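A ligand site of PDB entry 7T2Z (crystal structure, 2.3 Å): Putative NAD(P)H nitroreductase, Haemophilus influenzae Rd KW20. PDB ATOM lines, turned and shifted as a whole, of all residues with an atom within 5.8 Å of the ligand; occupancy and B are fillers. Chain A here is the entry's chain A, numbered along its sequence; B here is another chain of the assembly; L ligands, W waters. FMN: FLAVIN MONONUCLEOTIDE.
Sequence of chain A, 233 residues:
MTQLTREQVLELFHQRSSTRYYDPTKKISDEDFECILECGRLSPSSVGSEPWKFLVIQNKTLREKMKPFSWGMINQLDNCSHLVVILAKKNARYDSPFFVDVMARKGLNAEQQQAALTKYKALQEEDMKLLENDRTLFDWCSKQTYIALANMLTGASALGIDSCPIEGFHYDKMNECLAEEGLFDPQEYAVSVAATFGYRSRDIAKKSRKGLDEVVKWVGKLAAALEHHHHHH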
ATOM      1  N   ARG A  16      10.631   9.058  24.009  1.00  0.00           N
ATOM      2  CA  ARG A  16       9.465   8.291  23.614  1.00  0.00           C
ATOM      3  C   ARG A  16       9.846   6.827  23.526  1.00  0.00           C
ATOM      4  O   ARG A  16      10.807   6.472  22.830  1.00  0.00           O
ATOM      5  CB  ARG A  16       8.902   8.748  22.262  1.00  0.00           C
ATOM      6  CG  ARG A  16       7.573   8.056  21.903  1.00  0.00           C
ATOM      7  CD  ARG A  16       7.549   7.373  20.536  1.00  0.00           C
ATOM      8  NE  ARG A  16       8.777   6.637  20.229  1.00  0.00           N
ATOM      9  CZ  ARG A  16       8.945   5.330  20.399  1.00  0.00           C
ATOM     10  NH1 ARG A  16       7.967   4.573  20.886  1.00  0.00           N
ATOM     11  NH2 ARG A  16      10.107   4.779  20.086  1.00  0.00           N
ATOM     12  N   SER A  17       9.109   5.979  24.226  1.00  0.00           N
ATOM     13  CA  SER A  17       9.296   4.546  24.107  1.00  0.00           C
ATOM     14  C   SER A  17       7.934   3.882  24.165  1.00  0.00           C
ATOM     15  O   SER A  17       6.938   4.514  24.554  1.00  0.00           O
ATOM     16  CB  SER A  17      10.227   4.022  25.200  1.00  0.00           C
ATOM     17  OG  SER A  17       9.470   3.481  26.279  1.00  0.00           O
ATOM     18  N   SER A  18       7.900   2.610  23.772  1.00  0.00           N
ATOM     19  CA  SER A  18       6.639   1.877  23.685  1.00  0.00           C
ATOM     20  C   SER A  18       6.256   1.312  25.055  1.00  0.00           C
ATOM     21  O   SER A  18       6.953   0.461  25.602  1.00  0.00           O
ATOM     22  CB  SER A  18       6.771   0.764  22.644  1.00  0.00           C
ATOM     23  OG  SER A  18       7.011   1.272  21.342  1.00  0.00           O
ATOM     24  N   ARG A  20       4.216  -0.878  27.540  1.00  0.00           N
ATOM     25  CA  ARG A  20       3.437  -2.126  27.624  1.00  0.00           C
ATOM     26  C   ARG A  20       2.684  -2.278  28.940  1.00  0.00           C
ATOM     27  O   ARG A  20       1.969  -3.269  29.126  1.00  0.00           O
ATOM     28  CB  ARG A  20       4.350  -3.349  27.424  1.00  0.00           C
ATOM     29  CG  ARG A  20       4.603  -3.753  25.993  1.00  0.00           C
ATOM     30  CD  ARG A  20       5.563  -2.791  25.331  1.00  0.00           C
ATOM     31  NE  ARG A  20       5.874  -3.167  23.959  1.00  0.00           N
ATOM     32  CZ  ARG A  20       7.110  -3.183  23.449  1.00  0.00           C
ATOM     33  NH1 ARG A  20       8.133  -2.856  24.229  1.00  0.00           N
ATOM     34  NH2 ARG A  20       7.322  -3.532  22.181  1.00  0.00           N
ATOM     35  N   GLY A  72      -1.051  -8.389  20.809  1.00  0.00           N
ATOM     36  CA  GLY A  72      -0.092  -7.296  20.920  1.00  0.00           C
ATOM     37  C   GLY A  72      -0.430  -6.281  21.989  1.00  0.00           C
ATOM     38  O   GLY A  72       0.459  -5.536  22.427  1.00  0.00           O
ATOM     39  N   MET A  73      -1.702  -6.215  22.432  1.00  0.00           N
ATOM     40  CA  MET A  73      -2.080  -5.169  23.387  1.00  0.00           C
ATOM     41  C   MET A  73      -2.994  -5.688  24.491  1.00  0.00           C
ATOM     42  O   MET A  73      -3.682  -4.888  25.144  1.00  0.00           O
ATOM     43  CB  MET A  73      -2.752  -3.982  22.684  1.00  0.00           C
ATOM     44  CG  MET A  73      -3.935  -4.311  21.777  1.00  0.00           C
ATOM     45  SD  MET A  73      -4.888  -2.841  21.314  1.00  0.00           S
ATOM     46  CE  MET A  73      -5.982  -3.516  20.062  1.00  0.00           C
ATOM     47  N   GLN A  76      -2.467  -4.000  27.797  1.00  0.00           N
ATOM     48  CA  GLN A  76      -2.658  -2.562  27.758  1.00  0.00           C
ATOM     49  C   GLN A  76      -4.140  -2.206  27.643  1.00  0.00           C
ATOM     50  O   GLN A  76      -4.543  -1.125  28.093  1.00  0.00           O
ATOM     51  CB  GLN A  76      -1.897  -1.977  26.580  1.00  0.00           C
ATOM     52  CG  GLN A  76      -0.498  -2.487  26.453  1.00  0.00           C
ATOM     53  CD  GLN A  76       0.154  -2.028  25.161  1.00  0.00           C
ATOM     54  OE1 GLN A  76      -0.115  -0.917  24.680  1.00  0.00           O
ATOM     55  NE2 GLN A  76       1.016  -2.876  24.597  1.00  0.00           N
ATOM     56  N   TYR A 146       0.424   6.147   8.803  1.00  0.00           N
ATOM     57  CA  TYR A 146       1.559   5.954   9.692  1.00  0.00           C
ATOM     58  C   TYR A 146       2.267   7.266   9.964  1.00  0.00           C
ATOM     59  O   TYR A 146       2.960   7.372  10.990  1.00  0.00           O
ATOM     60  CB  TYR A 146       2.548   4.949   9.104  1.00  0.00           C
ATOM     61  CG  TYR A 146       2.144   3.523   9.391  1.00  0.00           C
ATOM     62  CD1 TYR A 146       0.919   3.033   8.971  1.00  0.00           C
ATOM     63  CD2 TYR A 146       2.991   2.676  10.121  1.00  0.00           C
ATOM     64  CE1 TYR A 146       0.541   1.715   9.231  1.00  0.00           C
ATOM     65  CE2 TYR A 146       2.633   1.376  10.397  1.00  0.00           C
ATOM     66  CZ  TYR A 146       1.423   0.896   9.953  1.00  0.00           C
ATOM     67  OH  TYR A 146       1.089  -0.392  10.252  1.00  0.00           O
ATOM     68  N   LEU A 149       0.122   8.531  12.699  1.00  0.00           N
ATOM     69  CA  LEU A 149       0.444   7.739  13.891  1.00  0.00           C
ATOM     70  C   LEU A 149       1.691   8.265  14.575  1.00  0.00           C
ATOM     71  O   LEU A 149       1.690   8.534  15.785  1.00  0.00           O
ATOM     72  CB  LEU A 149       0.630   6.276  13.515  1.00  0.00           C
ATOM     73  CG  LEU A 149       1.400   5.450  14.551  1.00  0.00           C
ATOM     74  CD1 LEU A 149       0.536   5.203  15.785  1.00  0.00           C
ATOM     75  CD2 LEU A 149       1.912   4.136  13.959  1.00  0.00           C
ATOM     76  N   LEU A 153       2.213   9.927  18.466  1.00  0.00           N
ATOM     77  CA  LEU A 153       3.143   9.421  19.470  1.00  0.00           C
ATOM     78  C   LEU A 153       4.104  10.515  19.917  1.00  0.00           C
ATOM     79  O   LEU A 153       4.366  10.688  21.115  1.00  0.00           O
ATOM     80  CB  LEU A 153       3.914   8.213  18.935  1.00  0.00           C
ATOM     81  CG  LEU A 153       3.134   7.037  18.316  1.00  0.00           C
ATOM     82  CD1 LEU A 153       4.045   5.945  17.814  1.00  0.00           C
ATOM     83  CD2 LEU A 153       2.125   6.474  19.303  1.00  0.00           C
ATOM     84  N   CYS A 164       1.992   3.464  23.015  1.00  0.00           N
ATOM     85  CA  CYS A 164       2.525   2.299  22.324  1.00  0.00           C
ATOM     86  C   CYS A 164       1.791   2.116  21.002  1.00  0.00           C
ATOM     87  O   CYS A 164       0.557   2.085  20.993  1.00  0.00           O
ATOM     88  CB  CYS A 164       2.376   1.031  23.178  1.00  0.00           C
ATOM     89  SG  CYS A 164       3.209  -0.411  22.455  1.00  0.00           S
ATOM     90  N   PRO A 165       2.497   2.016  19.879  1.00  0.00           N
ATOM     91  CA  PRO A 165       1.825   1.683  18.624  1.00  0.00           C
ATOM     92  C   PRO A 165       1.604   0.186  18.546  1.00  0.00           C
ATOM     93  O   PRO A 165       2.345  -0.587  19.151  1.00  0.00           O
ATOM     94  CB  PRO A 165       2.792   2.192  17.543  1.00  0.00           C
ATOM     95  CG  PRO A 165       4.143   2.255  18.227  1.00  0.00           C
ATOM     96  CD  PRO A 165       3.910   2.395  19.694  1.00  0.00           C
ATOM     97  N   ILE A 166       0.535  -0.219  17.834  1.00  0.00           N
ATOM     98  CA  ILE A 166      -0.017  -1.572  17.937  1.00  0.00           C
ATOM     99  C   ILE A 166      -0.296  -2.127  16.551  1.00  0.00           C
ATOM    100  O   ILE A 166      -1.125  -1.570  15.816  1.00  0.00           O
ATOM    101  CB  ILE A 166      -1.320  -1.605  18.779  1.00  0.00           C
ATOM    102  CG1 ILE A 166      -1.114  -1.058  20.200  1.00  0.00           C
ATOM    103  CG2 ILE A 166      -1.923  -3.014  18.816  1.00  0.00           C
ATOM    104  CD1 ILE A 166      -0.137  -1.850  21.052  1.00  0.00           C
ATOM    105  N   GLU A 167       0.369  -3.221  16.192  1.00  0.00           N
ATOM    106  CA  GLU A 167       0.035  -4.018  15.021  1.00  0.00           C
ATOM    107  C   GLU A 167      -0.327  -5.433  15.412  1.00  0.00           C
ATOM    108  O   GLU A 167      -0.701  -6.236  14.540  1.00  0.00           O
ATOM    109  CB  GLU A 167       1.200  -4.077  14.036  1.00  0.00           C
ATOM    110  CG  GLU A 167       1.337  -2.897  13.118  1.00  0.00           C
ATOM    111  CD  GLU A 167       2.478  -3.077  12.116  1.00  0.00           C
ATOM    112  OE1 GLU A 167       3.137  -4.136  12.169  1.00  0.00           O
ATOM    113  OE2 GLU A 167       2.714  -2.162  11.289  1.00  0.00           O
ATOM    114  N   GLY A 168      -0.230  -5.766  16.697  1.00  0.00           N
ATOM    115  CA  GLY A 168      -0.385  -7.137  17.137  1.00  0.00           C
ATOM    116  C   GLY A 168      -1.819  -7.498  17.392  1.00  0.00           C
ATOM    117  O   GLY A 168      -2.247  -7.597  18.542  1.00  0.00           O
ATOM    118  N   PHE A 169      -2.582  -7.688  16.313  1.00  0.00           N
ATOM    119  CA  PHE A 169      -3.956  -8.171  16.406  1.00  0.00           C
ATOM    120  C   PHE A 169      -4.311  -8.800  15.063  1.00  0.00           C
ATOM    121  O   PHE A 169      -3.661  -8.527  14.052  1.00  0.00           O
ATOM    122  CB  PHE A 169      -4.932  -7.048  16.777  1.00  0.00           C
ATOM    123  CG  PHE A 169      -4.832  -5.812  15.897  1.00  0.00           C
ATOM    124  CD1 PHE A 169      -4.176  -4.658  16.362  1.00  0.00           C
ATOM    125  CD2 PHE A 169      -5.405  -5.783  14.624  1.00  0.00           C
ATOM    126  CE1 PHE A 169      -4.088  -3.515  15.552  1.00  0.00           C
ATOM    127  CE2 PHE A 169      -5.327  -4.649  13.824  1.00  0.00           C
ATOM    128  CZ  PHE A 169      -4.660  -3.503  14.292  1.00  0.00           C
ATOM    129  N   VAL A 193      -3.728   0.659  11.688  1.00  0.00           N
ATOM    130  CA  VAL A 193      -2.802   0.462  12.793  1.00  0.00           C
ATOM    131  C   VAL A 193      -3.492   1.088  13.998  1.00  0.00           C
ATOM    132  O   VAL A 193      -4.449   1.850  13.843  1.00  0.00           O
ATOM    133  CB  VAL A 193      -1.424   1.131  12.495  1.00  0.00           C
ATOM    134  CG1 VAL A 193      -1.525   2.654  12.351  1.00  0.00           C
ATOM    135  CG2 VAL A 193      -0.346   0.737  13.527  1.00  0.00           C
ATOM    136  N   LYS A 207      16.861   2.600  25.038  1.00  0.00           N
ATOM    137  CA  LYS A 207      16.755   2.589  23.585  1.00  0.00           C
ATOM    138  C   LYS A 207      17.781   1.636  22.991  1.00  0.00           C
ATOM    139  O   LYS A 207      18.956   1.633  23.388  1.00  0.00           O
ATOM    140  CB  LYS A 207      16.949   3.989  23.011  1.00  0.00           C
ATOM    141  CG  LYS A 207      15.732   4.530  22.253  1.00  0.00           C
ATOM    142  CD  LYS A 207      14.478   4.314  23.094  1.00  0.00           C
ATOM    143  CE  LYS A 207      13.233   4.806  22.427  1.00  0.00           C
ATOM    144  NZ  LYS A 207      13.386   6.242  21.917  1.00  0.00           N
ATOM    145  N   SER A 208      17.323   0.817  22.053  1.00  0.00           N
ATOM    146  CA  SER A 208      18.191  -0.036  21.260  1.00  0.00           C
ATOM    147  C   SER A 208      17.860   0.233  19.811  1.00  0.00           C
ATOM    148  O   SER A 208      16.722  -0.005  19.382  1.00  0.00           O
ATOM    149  CB  SER A 208      17.994  -1.514  21.609  1.00  0.00           C
ATOM    150  OG  SER A 208      18.539  -2.376  20.621  1.00  0.00           O
ATOM    151  N   ARG A 209      18.837   0.757  19.048  1.00  0.00           N
ATOM    152  CA  ARG A 209      18.684   1.032  17.635  1.00  0.00           C
ATOM    153  C   ARG A 209      19.994   0.683  16.933  1.00  0.00           C
ATOM    154  O   ARG A 209      21.069   0.767  17.537  1.00  0.00           O
ATOM    155  CB  ARG A 209      18.333   2.493  17.359  1.00  0.00           C
ATOM    156  CG  ARG A 209      16.968   2.952  17.866  1.00  0.00           C
ATOM    157  CD  ARG A 209      15.828   2.276  17.107  1.00  0.00           C
ATOM    158  NE  ARG A 209      14.563   2.925  17.447  1.00  0.00           N
ATOM    159  CZ  ARG A 209      13.832   2.606  18.509  1.00  0.00           C
ATOM    160  NH1 ARG A 209      14.236   1.632  19.315  1.00  0.00           N
ATOM    161  NH2 ARG A 209      12.710   3.275  18.770  1.00  0.00           N
ATOM    162  N   LEU B  42      15.828   6.944  15.610  1.00  0.00           N
ATOM    163  CA  LEU B  42      15.185   6.655  16.883  1.00  0.00           C
ATOM    164  C   LEU B  42      13.727   6.269  16.732  1.00  0.00           C
ATOM    165  O   LEU B  42      13.065   6.017  17.748  1.00  0.00           O
ATOM    166  CB  LEU B  42      15.314   7.869  17.801  1.00  0.00           C
ATOM    167  CG  LEU B  42      16.745   8.307  18.171  1.00  0.00           C
ATOM    168  CD1 LEU B  42      16.761   9.580  18.984  1.00  0.00           C
ATOM    169  CD2 LEU B  42      17.488   7.211  18.906  1.00  0.00           C
ATOM    170  N   SER B  43      13.192   6.225  15.510  1.00  0.00           N
ATOM    171  CA  SER B  43      11.756   6.067  15.334  1.00  0.00           C
ATOM    172  C   SER B  43      11.302   4.668  15.771  1.00  0.00           C
ATOM    173  O   SER B  43      12.046   3.680  15.613  1.00  0.00           O
ATOM    174  CB  SER B  43      11.354   6.316  13.875  1.00  0.00           C
ATOM    175  OG  SER B  43      11.399   7.711  13.580  1.00  0.00           O
ATOM    176  N   PRO B  44      10.090   4.553  16.299  1.00  0.00           N
ATOM    177  CA  PRO B  44       9.529   3.227  16.574  1.00  0.00           C
ATOM    178  C   PRO B  44       9.410   2.453  15.272  1.00  0.00           C
ATOM    179  O   PRO B  44       9.483   2.993  14.180  1.00  0.00           O
ATOM    180  CB  PRO B  44       8.158   3.530  17.207  1.00  0.00           C
ATOM    181  CG  PRO B  44       7.780   4.881  16.659  1.00  0.00           C
ATOM    182  CD  PRO B  44       9.102   5.630  16.484  1.00  0.00           C
ATOM    183  N   SER B  45       9.149   1.161  15.416  1.00  0.00           N
ATOM    184  CA  SER B  45       9.282   0.257  14.297  1.00  0.00           C
ATOM    185  C   SER B  45       8.638  -1.073  14.701  1.00  0.00           C
ATOM    186  O   SER B  45       8.993  -1.641  15.736  1.00  0.00           O
ATOM    187  CB  SER B  45      10.756   0.103  13.957  1.00  0.00           C
ATOM    188  OG  SER B  45      10.927  -0.820  12.924  1.00  0.00           O
ATOM    189  N   SER B  46       7.681  -1.568  13.913  1.00  0.00           N
ATOM    190  CA  SER B  46       7.063  -2.855  14.209  1.00  0.00           C
ATOM    191  C   SER B  46       8.129  -3.899  14.516  1.00  0.00           C
ATOM    192  O   SER B  46       9.091  -4.062  13.755  1.00  0.00           O
ATOM    193  CB  SER B  46       6.199  -3.319  13.044  1.00  0.00           C
ATOM    194  OG  SER B  46       5.545  -4.520  13.359  1.00  0.00           O
ATOM    195  N   VAL B  47       7.958  -4.592  15.660  1.00  0.00           N
ATOM    196  CA  VAL B  47       8.859  -5.615  16.206  1.00  0.00           C
ATOM    197  C   VAL B  47      10.328  -5.197  16.124  1.00  0.00           C
ATOM    198  O   VAL B  47      11.210  -6.039  15.918  1.00  0.00           O
ATOM    199  CB  VAL B  47       8.637  -7.004  15.548  1.00  0.00           C
ATOM    200  CG1 VAL B  47       7.243  -7.546  15.897  1.00  0.00           C
ATOM    201  CG2 VAL B  47       8.874  -7.017  14.012  1.00  0.00           C
ATOM    202  N   GLY B  48      10.600  -3.901  16.327  1.00  0.00           N
ATOM    203  CA  GLY B  48      11.966  -3.385  16.310  1.00  0.00           C
ATOM    204  C   GLY B  48      12.690  -3.637  15.009  1.00  0.00           C
ATOM    205  O   GLY B  48      13.926  -3.742  14.991  1.00  0.00           O
ATOM    206  N   LYS B 106      18.800  -8.074  20.156  1.00  0.00           N
ATOM    207  CA  LYS B 106      17.996  -8.168  21.378  1.00  0.00           C
ATOM    208  C   LYS B 106      18.490  -9.259  22.323  1.00  0.00           C
ATOM    209  O   LYS B 106      17.945  -9.408  23.423  1.00  0.00           O
ATOM    210  CB  LYS B 106      16.519  -8.409  21.040  1.00  0.00           C
ATOM    211  CG  LYS B 106      15.830  -7.256  20.284  1.00  0.00           C
ATOM    212  CD  LYS B 106      16.328  -5.882  20.777  1.00  0.00           C
ATOM    213  CE  LYS B 106      15.241  -4.826  20.673  1.00  0.00           C
ATOM    214  NZ  LYS B 106      15.260  -3.881  21.823  1.00  0.00           N
ATOM    215  N   GLN B 144       6.624   1.399   8.019  1.00  0.00           N
ATOM    216  CA  GLN B 144       7.506   1.777   9.123  1.00  0.00           C
ATOM    217  C   GLN B 144       8.381   2.962   8.737  1.00  0.00           C
ATOM    218  O   GLN B 144       8.605   3.860   9.553  1.00  0.00           O
ATOM    219  CB  GLN B 144       8.382   0.592   9.586  1.00  0.00           C
ATOM    220  CG  GLN B 144       7.748  -0.808   9.592  1.00  0.00           C
ATOM    221  CD  GLN B 144       6.488  -0.906  10.449  1.00  0.00           C
ATOM    222  OE1 GLN B 144       6.448  -0.438  11.590  1.00  0.00           O
ATOM    223  NE2 GLN B 144       5.434  -1.505   9.881  1.00  0.00           N
ATOM    224  N   ILE B 147       6.959   6.344   9.320  1.00  0.00           N
ATOM    225  CA  ILE B 147       7.130   6.863  10.676  1.00  0.00           C
ATOM    226  C   ILE B 147       8.431   7.643  10.765  1.00  0.00           C
ATOM    227  O   ILE B 147       8.460   8.782  11.249  1.00  0.00           O
ATOM    228  CB  ILE B 147       7.101   5.712  11.721  1.00  0.00           C
ATOM    229  CG1 ILE B 147       5.764   4.977  11.735  1.00  0.00           C
ATOM    230  CG2 ILE B 147       7.379   6.261  13.128  1.00  0.00           C
ATOM    231  CD1 ILE B 147       5.756   3.880  12.770  1.00  0.00           C
HETATM  232  N1  FMN L   1       4.471  -3.149  20.549  1.00  0.00           N
HETATM  233  C2  FMN L   1       3.548  -3.874  21.199  1.00  0.00           C
HETATM  234  O2  FMN L   1       3.663  -4.141  22.407  1.00  0.00           O
HETATM  235  N3  FMN L   1       2.445  -4.372  20.564  1.00  0.00           N
HETATM  236  C4  FMN L   1       2.185  -4.132  19.232  1.00  0.00           C
HETATM  237  O4  FMN L   1       1.160  -4.603  18.723  1.00  0.00           O
HETATM  238  C4A FMN L   1       3.114  -3.304  18.534  1.00  0.00           C
HETATM  239  N5  FMN L   1       2.882  -2.978  17.271  1.00  0.00           N
HETATM  240  C5A FMN L   1       3.676  -2.014  16.712  1.00  0.00           C
HETATM  241  C6  FMN L   1       3.277  -1.428  15.492  1.00  0.00           C
HETATM  242  C7  FMN L   1       3.955  -0.352  14.950  1.00  0.00           C
HETATM  243  C7M FMN L   1       3.448   0.330  13.696  1.00  0.00           C
HETATM  244  C8  FMN L   1       5.101   0.134  15.597  1.00  0.00           C
HETATM  245  C8M FMN L   1       5.800   1.360  15.068  1.00  0.00           C
HETATM  246  C9  FMN L   1       5.542  -0.463  16.755  1.00  0.00           C
HETATM  247  C9A FMN L   1       4.816  -1.499  17.367  1.00  0.00           C
HETATM  248  N10 FMN L   1       5.136  -2.010  18.627  1.00  0.00           N
HETATM  249  C10 FMN L   1       4.248  -2.821  19.296  1.00  0.00           C
HETATM  250  C1' FMN L   1       6.271  -1.425  19.355  1.00  0.00           C
HETATM  251  C2' FMN L   1       7.610  -1.892  18.816  1.00  0.00           C
HETATM  252  O2' FMN L   1       7.860  -3.230  19.234  1.00  0.00           O
HETATM  253  C3' FMN L   1       8.691  -0.933  19.305  1.00  0.00           C
HETATM  254  O3' FMN L   1       8.489   0.310  18.633  1.00  0.00           O
HETATM  255  C4' FMN L   1      10.143  -1.333  19.041  1.00  0.00           C
HETATM  256  O4' FMN L   1      10.436  -2.581  19.675  1.00  0.00           O
HETATM  257  C5' FMN L   1      11.124  -0.281  19.528  1.00  0.00           C
HETATM  258  O5' FMN L   1      10.916  -0.027  20.945  1.00  0.00           O
HETATM  259  P   FMN L   1      10.604   1.486  21.426  1.00  0.00           P
HETATM  260  O1P FMN L   1      11.764   2.377  21.129  1.00  0.00           O
HETATM  261  O2P FMN L   1       9.361   1.955  20.667  1.00  0.00           O
HETATM  262  O3P FMN L   1      10.343   1.325  22.909  1.00  0.00           O
HETATM  263  O   HOH W   1      10.613  -2.689  22.611  1.00  0.00           O
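O3' of the ligand sits close to N of Ser 45 of chain B, 3.4 Å away.
An oxygen (O4) of the ligand is in hydrogen-bond range of the backbone NH (N) of Gly 168 (2.7 Å).
O of Gly 72 is in hydrogen-bond range of N3 of the ligand (3.0 Å).
A nitrogen (N1) of the ligand is in hydrogen-bond range of the side-chain sulfur (SG) of Cys 164, at 3.6 Å.
The side-chain hydroxyl (OG) of Ser 18 is in hydrogen-bond range of an oxygen (O2P) of the ligand, 2.5 Å away.
O2 of the ligand lies within hydrogen-bond range of NE of Arg 20 (2.9 Å).
N of Ser 18 is in hydrogen-bond range of O3P of the ligand (2.9 Å).
The guanidinium group (NH2) of Arg 209 is in salt-bridge range of an oxygen (O1P) of the ligand, at 2.7 Å.
An oxygen (O2P) of the ligand lies within salt-bridge range of the guanidinium group (NH1) of Arg 16 (3.0 Å).
N of Glu 167 is in hydrogen-bond range of N5 of the ligand, at 2.7 Å.
The side-chain carboxylate (OE2) of Glu 167 sits at hydrogen-bond distance from the side-chain amide nitrogen (NE2) of Gln 144 of chain B.
The guanidinium group of Arg 209 lies within hydrogen-bond range of the backbone carbonyl oxygen of Leu 42 of chain B, 2.9 Å away.
The side-chain amino group (NZ) of Lys 207 is in hydrogen-bond range of the backbone carbonyl oxygen (O) of Arg 16, at 2.7 Å.
The side-chain hydroxyl (OG) of Ser 18 sits at hydrogen-bond distance from the guanidinium group (NH1) of Arg 16, at 3.5 Å.
NE of Arg 209 lies within hydrogen-bond range of O of Ser 43 of chain B (3.2 Å).
The backbone NH (N) of Ser 46 of chain B is in hydrogen-bond range of the side-chain amide oxygen (OE1) of Gln 144 of chain B (2.9 Å).
The backbone carbonyl oxygen of Gly 72 sits at hydrogen-bond distance from the side-chain amide nitrogen of Gln 76 (3.5 Å).
The side-chain carboxylate (OE2) of Glu 167 sits at hydrogen-bond distance from the side-chain hydroxyl (OH) of Tyr 146.
O of Pro 165 sits close to N5 of the ligand (3.1 Å).
Ser 17 touches the ligand.
NE2 of Gln 76 touches O2 of the ligand, 3.7 Å away.
CE2 of Tyr 146 touches C7M of the ligand, at 3.6 Å.
Ile 166 touches the ligand (CA to N5, 3.3 Å).
CG2 of Val 193 touches C7M of the ligand (3.8 Å).
Lys 207 touches the ligand.
CB of Pro 44 of chain B touches O3' of the ligand, 3.5 Å away.
N of Ser 46 of chain B touches C8 of the ligand, at 3.5 Å.
Val 47 of chain B touches the ligand.
N of Gly 48 of chain B touches O4' of the ligand, 3.6 Å away.
Gln 144 of chain B touches the ligand (OE1 to C7M, 3.7 Å).
Ile 147 of chain B touches the ligand.
Hydrophobic or aromatic side chains within 4 Å of the ligand: Tyr 146, Pro 165, Ile 166, Val 193, Pro 44 of chain B and Ile 147 of chain B.
22 residues have an atom within 4 Å of the ligand: Arg 16, Ser 17, Ser 18, Arg 20, Gly 72, Gln 76, Tyr 146, Cys 164, Pro 165, Ile 166, Glu 167, Gly 168, Val 193, Lys 207, Arg 209, Pro 44 of chain B, Ser 45 of chain B, Ser 46 of chain B, Val 47 of chain B, Gly 48 of chain B, Gln 144 of chain B and Ile 147 of chain B.
The nearest printed residue that does not touch the ligand is Leu 149 (4.1 Å).
Water W1 lies within hydrogen-bond range of O4' of the ligand (2.9 Å) and NH1 of Arg 20 (3.0 Å).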
